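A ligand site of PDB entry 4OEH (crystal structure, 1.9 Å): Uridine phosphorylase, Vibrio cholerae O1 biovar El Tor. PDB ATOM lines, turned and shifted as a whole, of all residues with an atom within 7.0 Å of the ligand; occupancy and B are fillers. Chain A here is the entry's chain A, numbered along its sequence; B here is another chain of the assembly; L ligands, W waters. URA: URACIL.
Merely in contact with the ligand: Thr 93, Thr 94, Gly 95, Phe 161, Phe 194, Glu 195, Met 196 and Ile 220. Ten residues have an atom within 4 Å of the ligand: Thr 93, Thr 94, Gly 95, Phe 161, Gln 165, Arg 167, Phe 194, Glu 195, Met 196 and Ile 220.
The side-chain amide oxygen (OE1) of Gln 165 sits at hydrogen-bond distance from a nitrogen (N3) of the ligand (2.8 Å). The guanidinium group of Arg 167 lies within hydrogen-bond range of an oxygen (O4) of the ligand.
Water W1 lies within hydrogen-bond range of O4 of the ligand (2.8 Å), NH2 of Arg 222 (2.9 Å) and OE1 of Gln 165 (3.0 Å).
The backbone NH (N) of Ser 158 sits at hydrogen-bond distance from the backbone carbonyl oxygen (O) of Glu 195. The side-chain hydroxyl of Thr 94 lies within hydrogen-bond range of the backbone carbonyl oxygen of Phe 194, 2.6 Å away. OE1 of Gln 165 sits at hydrogen-bond distance from NH1 of Arg 167, 3.0 Å away. NE2 of Gln 165 sits at hydrogen-bond distance from O of Thr 160. The backbone NH of Ala 96 sits at hydrogen-bond distance from the backbone carbonyl oxygen of Ile 220 (2.8 Å). N of Thr 94 lies within hydrogen-bond range of O of Gly 217 (3.1 Å). The guanidinium group (NH2) of Arg 222 is in hydrogen-bond range of the backbone carbonyl oxygen (O) of Gln 165 (2.7 Å). The backbone carbonyl oxygen (O) of Thr 94 sits at hydrogen-bond distance from the backbone NH (N) of Ile 219, at 3.0 Å.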
ATOM      1  N   THR A  93       8.563  -8.123 -22.338  1.00  0.00           N
ATOM      2  CA  THR A  93       7.467  -7.236 -22.680  1.00  0.00           C
ATOM      3  C   THR A  93       7.692  -6.731 -24.099  1.00  0.00           C
ATOM      4  O   THR A  93       8.801  -6.819 -24.618  1.00  0.00           O
ATOM      5  CB  THR A  93       7.441  -6.031 -21.726  1.00  0.00           C
ATOM      6  OG1 THR A  93       8.680  -5.315 -21.843  1.00  0.00           O
ATOM      7  CG2 THR A  93       7.263  -6.505 -20.275  1.00  0.00           C
ATOM      8  N   THR A  94       6.645  -6.194 -24.715  1.00  0.00           N
ATOM      9  CA  THR A  94       6.762  -5.699 -26.087  1.00  0.00           C
ATOM     10  C   THR A  94       5.715  -4.651 -26.414  1.00  0.00           C
ATOM     11  O   THR A  94       4.668  -4.587 -25.776  1.00  0.00           O
ATOM     12  CB  THR A  94       6.691  -6.844 -27.138  1.00  0.00           C
ATOM     13  OG1 THR A  94       6.984  -6.304 -28.426  1.00  0.00           O
ATOM     14  CG2 THR A  94       5.313  -7.523 -27.166  1.00  0.00           C
ATOM     15  N   GLY A  95       6.023  -3.816 -27.415  1.00  0.00           N
ATOM     16  CA  GLY A  95       5.081  -2.849 -27.921  1.00  0.00           C
ATOM     17  C   GLY A  95       4.586  -3.327 -29.261  1.00  0.00           C
ATOM     18  O   GLY A  95       5.383  -3.528 -30.168  1.00  0.00           O
ATOM     19  N   ALA A  96       3.285  -3.533 -29.391  1.00  0.00           N
ATOM     20  CA  ALA A  96       2.701  -3.877 -30.697  1.00  0.00           C
ATOM     21  C   ALA A  96       2.617  -2.665 -31.610  1.00  0.00           C
ATOM     22  O   ALA A  96       2.452  -1.515 -31.137  1.00  0.00           O
ATOM     23  CB  ALA A  96       1.335  -4.517 -30.528  1.00  0.00           C
ATOM     24  N   ALA A 156      10.482  -6.550 -34.740  1.00  0.00           N
ATOM     25  CA  ALA A 156      11.572  -5.597 -35.001  1.00  0.00           C
ATOM     26  C   ALA A 156      12.345  -5.428 -33.683  1.00  0.00           C
ATOM     27  O   ALA A 156      11.762  -5.075 -32.667  1.00  0.00           O
ATOM     28  CB  ALA A 156      11.031  -4.273 -35.526  1.00  0.00           C
ATOM     29  N   SER A 158      15.341  -3.696 -31.631  1.00  0.00           N
ATOM     30  CA  SER A 158      16.084  -2.440 -31.726  1.00  0.00           C
ATOM     31  C   SER A 158      17.132  -2.238 -30.616  1.00  0.00           C
ATOM     32  O   SER A 158      16.888  -2.588 -29.471  1.00  0.00           O
ATOM     33  CB  SER A 158      15.093  -1.265 -31.705  1.00  0.00           C
ATOM     34  OG  SER A 158      15.768  -0.025 -31.606  1.00  0.00           O
ATOM     35  N   THR A 160      17.772   0.638 -29.527  1.00  0.00           N
ATOM     36  CA  THR A 160      17.247   1.725 -28.700  1.00  0.00           C
ATOM     37  C   THR A 160      15.751   1.575 -28.456  1.00  0.00           C
ATOM     38  O   THR A 160      15.038   0.926 -29.224  1.00  0.00           O
ATOM     39  CB  THR A 160      17.511   3.131 -29.299  1.00  0.00           C
ATOM     40  OG1 THR A 160      16.928   3.233 -30.597  1.00  0.00           O
ATOM     41  CG2 THR A 160      19.032   3.417 -29.406  1.00  0.00           C
ATOM     42  N   PHE A 161      15.287   2.178 -27.354  1.00  0.00           N
ATOM     43  CA  PHE A 161      13.876   2.203 -27.048  1.00  0.00           C
ATOM     44  C   PHE A 161      13.240   3.413 -27.736  1.00  0.00           C
ATOM     45  O   PHE A 161      12.033   3.412 -28.025  1.00  0.00           O
ATOM     46  CB  PHE A 161      13.700   2.299 -25.523  1.00  0.00           C
ATOM     47  CG  PHE A 161      12.278   2.291 -25.067  1.00  0.00           C
ATOM     48  CD1 PHE A 161      11.603   1.081 -24.835  1.00  0.00           C
ATOM     49  CD2 PHE A 161      11.595   3.487 -24.832  1.00  0.00           C
ATOM     50  CE1 PHE A 161      10.290   1.071 -24.404  1.00  0.00           C
ATOM     51  CE2 PHE A 161      10.282   3.478 -24.402  1.00  0.00           C
ATOM     52  CZ  PHE A 161       9.624   2.280 -24.177  1.00  0.00           C
ATOM     53  N   GLN A 165      12.769   2.972 -32.434  1.00  0.00           N
ATOM     54  CA  GLN A 165      11.351   2.600 -32.406  1.00  0.00           C
ATOM     55  C   GLN A 165      10.505   3.821 -32.817  1.00  0.00           C
ATOM     56  O   GLN A 165       9.311   3.904 -32.542  1.00  0.00           O
ATOM     57  CB  GLN A 165      10.941   2.061 -31.015  1.00  0.00           C
ATOM     58  CG  GLN A 165      11.902   0.984 -30.513  1.00  0.00           C
ATOM     59  CD  GLN A 165      11.392   0.149 -29.350  1.00  0.00           C
ATOM     60  OE1 GLN A 165      10.215   0.202 -28.976  1.00  0.00           O
ATOM     61  NE2 GLN A 165      12.276  -0.666 -28.783  1.00  0.00           N
ATOM     62  N   ARG A 167      10.213   6.910 -31.799  1.00  0.00           N
ATOM     63  CA  ARG A 167       9.538   7.746 -30.803  1.00  0.00           C
ATOM     64  C   ARG A 167      10.061   9.159 -30.937  1.00  0.00           C
ATOM     65  O   ARG A 167      11.275   9.380 -30.953  1.00  0.00           O
ATOM     66  CB  ARG A 167       9.787   7.223 -29.380  1.00  0.00           C
ATOM     67  CG  ARG A 167       8.887   6.067 -28.949  1.00  0.00           C
ATOM     68  CD  ARG A 167       9.182   5.599 -27.522  1.00  0.00           C
ATOM     69  NE  ARG A 167       8.134   4.677 -27.052  1.00  0.00           N
ATOM     70  CZ  ARG A 167       8.164   3.358 -27.195  1.00  0.00           C
ATOM     71  NH1 ARG A 167       9.208   2.757 -27.759  1.00  0.00           N
ATOM     72  NH2 ARG A 167       7.145   2.633 -26.760  1.00  0.00           N
ATOM     73  N   PHE A 194       7.774  -4.212 -31.544  1.00  0.00           N
ATOM     74  CA  PHE A 194       9.131  -3.813 -31.174  1.00  0.00           C
ATOM     75  C   PHE A 194       9.559  -4.436 -29.832  1.00  0.00           C
ATOM     76  O   PHE A 194       8.781  -4.462 -28.875  1.00  0.00           O
ATOM     77  CB  PHE A 194       9.242  -2.285 -31.000  1.00  0.00           C
ATOM     78  CG  PHE A 194       9.402  -1.512 -32.276  1.00  0.00           C
ATOM     79  CD1 PHE A 194      10.572  -1.605 -33.038  1.00  0.00           C
ATOM     80  CD2 PHE A 194       8.419  -0.608 -32.693  1.00  0.00           C
ATOM     81  CE1 PHE A 194      10.738  -0.865 -34.207  1.00  0.00           C
ATOM     82  CE2 PHE A 194       8.584   0.145 -33.856  1.00  0.00           C
ATOM     83  CZ  PHE A 194       9.743   0.022 -34.609  1.00  0.00           C
ATOM     84  N   GLU A 195      10.781  -4.965 -29.782  1.00  0.00           N
ATOM     85  CA  GLU A 195      11.491  -5.167 -28.520  1.00  0.00           C
ATOM     86  C   GLU A 195      13.005  -4.990 -28.723  1.00  0.00           C
ATOM     87  O   GLU A 195      13.429  -4.489 -29.773  1.00  0.00           O
ATOM     88  CB  GLU A 195      11.109  -6.473 -27.778  1.00  0.00           C
ATOM     89  CG  GLU A 195      11.188  -7.742 -28.598  1.00  0.00           C
ATOM     90  CD  GLU A 195      12.619  -8.130 -28.900  1.00  0.00           C
ATOM     91  OE1 GLU A 195      13.084  -7.781 -29.997  1.00  0.00           O
ATOM     92  OE2 GLU A 195      13.289  -8.712 -28.021  1.00  0.00           O
ATOM     93  N   MET A 196      13.830  -5.358 -27.750  1.00  0.00           N
ATOM     94  CA  MET A 196      15.233  -4.930 -27.822  1.00  0.00           C
ATOM     95  C   MET A 196      16.275  -6.020 -27.655  1.00  0.00           C
ATOM     96  O   MET A 196      17.463  -5.727 -27.552  1.00  0.00           O
ATOM     97  CB  MET A 196      15.498  -3.774 -26.834  1.00  0.00           C
ATOM     98  CG  MET A 196      14.613  -2.539 -27.046  1.00  0.00           C
ATOM     99  SD  MET A 196      14.867  -1.253 -25.808  1.00  0.00           S
ATOM    100  CE  MET A 196      16.633  -0.931 -25.995  1.00  0.00           C
ATOM    101  N   GLU A 197      15.859  -7.297 -27.671  1.00  0.00           N
ATOM    102  CA  GLU A 197      16.794  -8.394 -27.415  1.00  0.00           C
ATOM    103  C   GLU A 197      16.772  -9.569 -28.411  1.00  0.00           C
ATOM    104  O   GLU A 197      17.751 -10.317 -28.508  1.00  0.00           O
ATOM    105  CB  GLU A 197      16.594  -8.939 -25.982  1.00  0.00           C
ATOM    106  CG  GLU A 197      16.978  -7.965 -24.866  1.00  0.00           C
ATOM    107  CD  GLU A 197      15.880  -6.955 -24.553  1.00  0.00           C
ATOM    108  OE1 GLU A 197      14.715  -7.158 -24.929  1.00  0.00           O
ATOM    109  OE2 GLU A 197      16.199  -5.927 -23.911  1.00  0.00           O
ATOM    110  N   GLY A 217       4.686 -10.665 -24.021  1.00  0.00           N
ATOM    111  CA  GLY A 217       3.364 -10.154 -23.663  1.00  0.00           C
ATOM    112  C   GLY A 217       3.269  -8.716 -24.116  1.00  0.00           C
ATOM    113  O   GLY A 217       4.195  -7.927 -23.891  1.00  0.00           O
ATOM    114  N   ILE A 219       2.412  -5.120 -23.837  1.00  0.00           N
ATOM    115  CA  ILE A 219       2.153  -4.149 -22.761  1.00  0.00           C
ATOM    116  C   ILE A 219       1.681  -2.787 -23.282  1.00  0.00           C
ATOM    117  O   ILE A 219       1.078  -2.002 -22.534  1.00  0.00           O
ATOM    118  CB  ILE A 219       3.354  -3.996 -21.769  1.00  0.00           C
ATOM    119  CG1 ILE A 219       4.598  -3.424 -22.455  1.00  0.00           C
ATOM    120  CG2 ILE A 219       3.663  -5.337 -21.107  1.00  0.00           C
ATOM    121  CD1 ILE A 219       5.541  -2.691 -21.514  1.00  0.00           C
ATOM    122  N   ILE A 220       1.945  -2.505 -24.553  1.00  0.00           N
ATOM    123  CA  ILE A 220       1.466  -1.303 -25.197  1.00  0.00           C
ATOM    124  C   ILE A 220       1.215  -1.579 -26.687  1.00  0.00           C
ATOM    125  O   ILE A 220       1.815  -2.485 -27.254  1.00  0.00           O
ATOM    126  CB  ILE A 220       2.435  -0.109 -24.994  1.00  0.00           C
ATOM    127  CG1 ILE A 220       1.662   1.210 -24.943  1.00  0.00           C
ATOM    128  CG2 ILE A 220       3.528  -0.083 -26.054  1.00  0.00           C
ATOM    129  CD1 ILE A 220       2.347   2.324 -24.175  1.00  0.00           C
ATOM    130  N   ASN A 221       0.292  -0.835 -27.285  1.00  0.00           N
ATOM    131  CA  ASN A 221       0.145  -0.805 -28.732  1.00  0.00           C
ATOM    132  C   ASN A 221       0.343   0.627 -29.231  1.00  0.00           C
ATOM    133  O   ASN A 221      -0.385   1.537 -28.822  1.00  0.00           O
ATOM    134  CB  ASN A 221      -1.217  -1.349 -29.175  1.00  0.00           C
ATOM    135  CG  ASN A 221      -1.347  -1.419 -30.690  1.00  0.00           C
ATOM    136  OD1 ASN A 221      -1.020  -0.473 -31.405  1.00  0.00           O
ATOM    137  ND2 ASN A 221      -1.832  -2.545 -31.196  1.00  0.00           N
ATOM    138  N   ARG A 222       1.317   0.815 -30.115  1.00  0.00           N
ATOM    139  CA  ARG A 222       1.732   2.138 -30.589  1.00  0.00           C
ATOM    140  C   ARG A 222       0.673   2.851 -31.430  1.00  0.00           C
ATOM    141  O   ARG A 222       0.732   4.056 -31.597  1.00  0.00           O
ATOM    142  CB  ARG A 222       3.063   2.056 -31.357  1.00  0.00           C
ATOM    143  CG  ARG A 222       4.255   1.541 -30.542  1.00  0.00           C
ATOM    144  CD  ARG A 222       4.818   2.636 -29.648  1.00  0.00           C
ATOM    145  NE  ARG A 222       5.225   3.815 -30.423  1.00  0.00           N
ATOM    146  CZ  ARG A 222       6.407   3.963 -31.023  1.00  0.00           C
ATOM    147  NH1 ARG A 222       6.669   5.064 -31.711  1.00  0.00           N
ATOM    148  NH2 ARG A 222       7.323   3.003 -30.919  1.00  0.00           N
ATOM    149  N   PHE B   6       9.868   6.573 -18.269  1.00  0.00           N
ATOM    150  CA  PHE B   6       9.385   5.188 -18.427  1.00  0.00           C
ATOM    151  C   PHE B   6      10.161   4.132 -17.636  1.00  0.00           C
ATOM    152  O   PHE B   6       9.551   3.275 -16.999  1.00  0.00           O
ATOM    153  CB  PHE B   6       9.298   4.802 -19.905  1.00  0.00           C
ATOM    154  CG  PHE B   6       8.514   3.529 -20.155  1.00  0.00           C
ATOM    155  CD1 PHE B   6       7.122   3.554 -20.282  1.00  0.00           C
ATOM    156  CD2 PHE B   6       9.173   2.295 -20.275  1.00  0.00           C
ATOM    157  CE1 PHE B   6       6.406   2.382 -20.509  1.00  0.00           C
ATOM    158  CE2 PHE B   6       8.457   1.123 -20.502  1.00  0.00           C
ATOM    159  CZ  PHE B   6       7.071   1.168 -20.623  1.00  0.00           C
ATOM    160  N   HIS B   7      11.487   4.190 -17.679  1.00  0.00           N
ATOM    161  CA  HIS B   7      12.342   3.155 -17.076  1.00  0.00           C
ATOM    162  C   HIS B   7      12.908   3.548 -15.743  1.00  0.00           C
ATOM    163  O   HIS B   7      12.863   2.763 -14.789  1.00  0.00           O
ATOM    164  CB  HIS B   7      13.465   2.756 -18.032  1.00  0.00           C
ATOM    165  CG  HIS B   7      12.985   2.149 -19.340  1.00  0.00           C
ATOM    166  ND1 HIS B   7      12.606   2.900 -20.384  1.00  0.00           N
ATOM    167  CD2 HIS B   7      12.845   0.810 -19.732  1.00  0.00           C
ATOM    168  CE1 HIS B   7      12.233   2.092 -21.407  1.00  0.00           C
ATOM    169  NE2 HIS B   7      12.376   0.813 -20.996  1.00  0.00           N
ATOM    170  N   ARG B  47      14.955  -2.458 -12.676  1.00  0.00           N
ATOM    171  CA  ARG B  47      15.816  -3.210 -13.604  1.00  0.00           C
ATOM    172  C   ARG B  47      17.282  -2.887 -13.285  1.00  0.00           C
ATOM    173  O   ARG B  47      17.679  -2.908 -12.124  1.00  0.00           O
ATOM    174  CB  ARG B  47      15.454  -2.904 -15.073  1.00  0.00           C
ATOM    175  CG  ARG B  47      14.060  -3.330 -15.511  1.00  0.00           C
ATOM    176  CD  ARG B  47      13.854  -3.008 -16.979  1.00  0.00           C
ATOM    177  NE  ARG B  47      12.625  -3.578 -17.568  1.00  0.00           N
ATOM    178  CZ  ARG B  47      12.573  -4.638 -18.375  1.00  0.00           C
ATOM    179  NH1 ARG B  47      13.680  -5.317 -18.706  1.00  0.00           N
ATOM    180  NH2 ARG B  47      11.403  -5.036 -18.851  1.00  0.00           N
HETATM  181  N1  URA L   1       9.584  -2.860 -25.097  1.00  0.00           N
HETATM  182  C2  URA L   1       9.984  -2.153 -26.189  1.00  0.00           C
HETATM  183  O2  URA L   1      11.132  -2.324 -26.657  1.00  0.00           O
HETATM  184  N3  URA L   1       9.168  -1.263 -26.775  1.00  0.00           N
HETATM  185  C4  URA L   1       7.927  -1.052 -26.290  1.00  0.00           C
HETATM  186  O4  URA L   1       7.160  -0.217 -26.848  1.00  0.00           O
HETATM  187  C5  URA L   1       7.482  -1.764 -25.161  1.00  0.00           C
HETATM  188  C6  URA L   1       8.352  -2.689 -24.569  1.00  0.00           C
HETATM  189  O   HOH W   1       7.293   0.372 -29.589  1.00  0.00           O
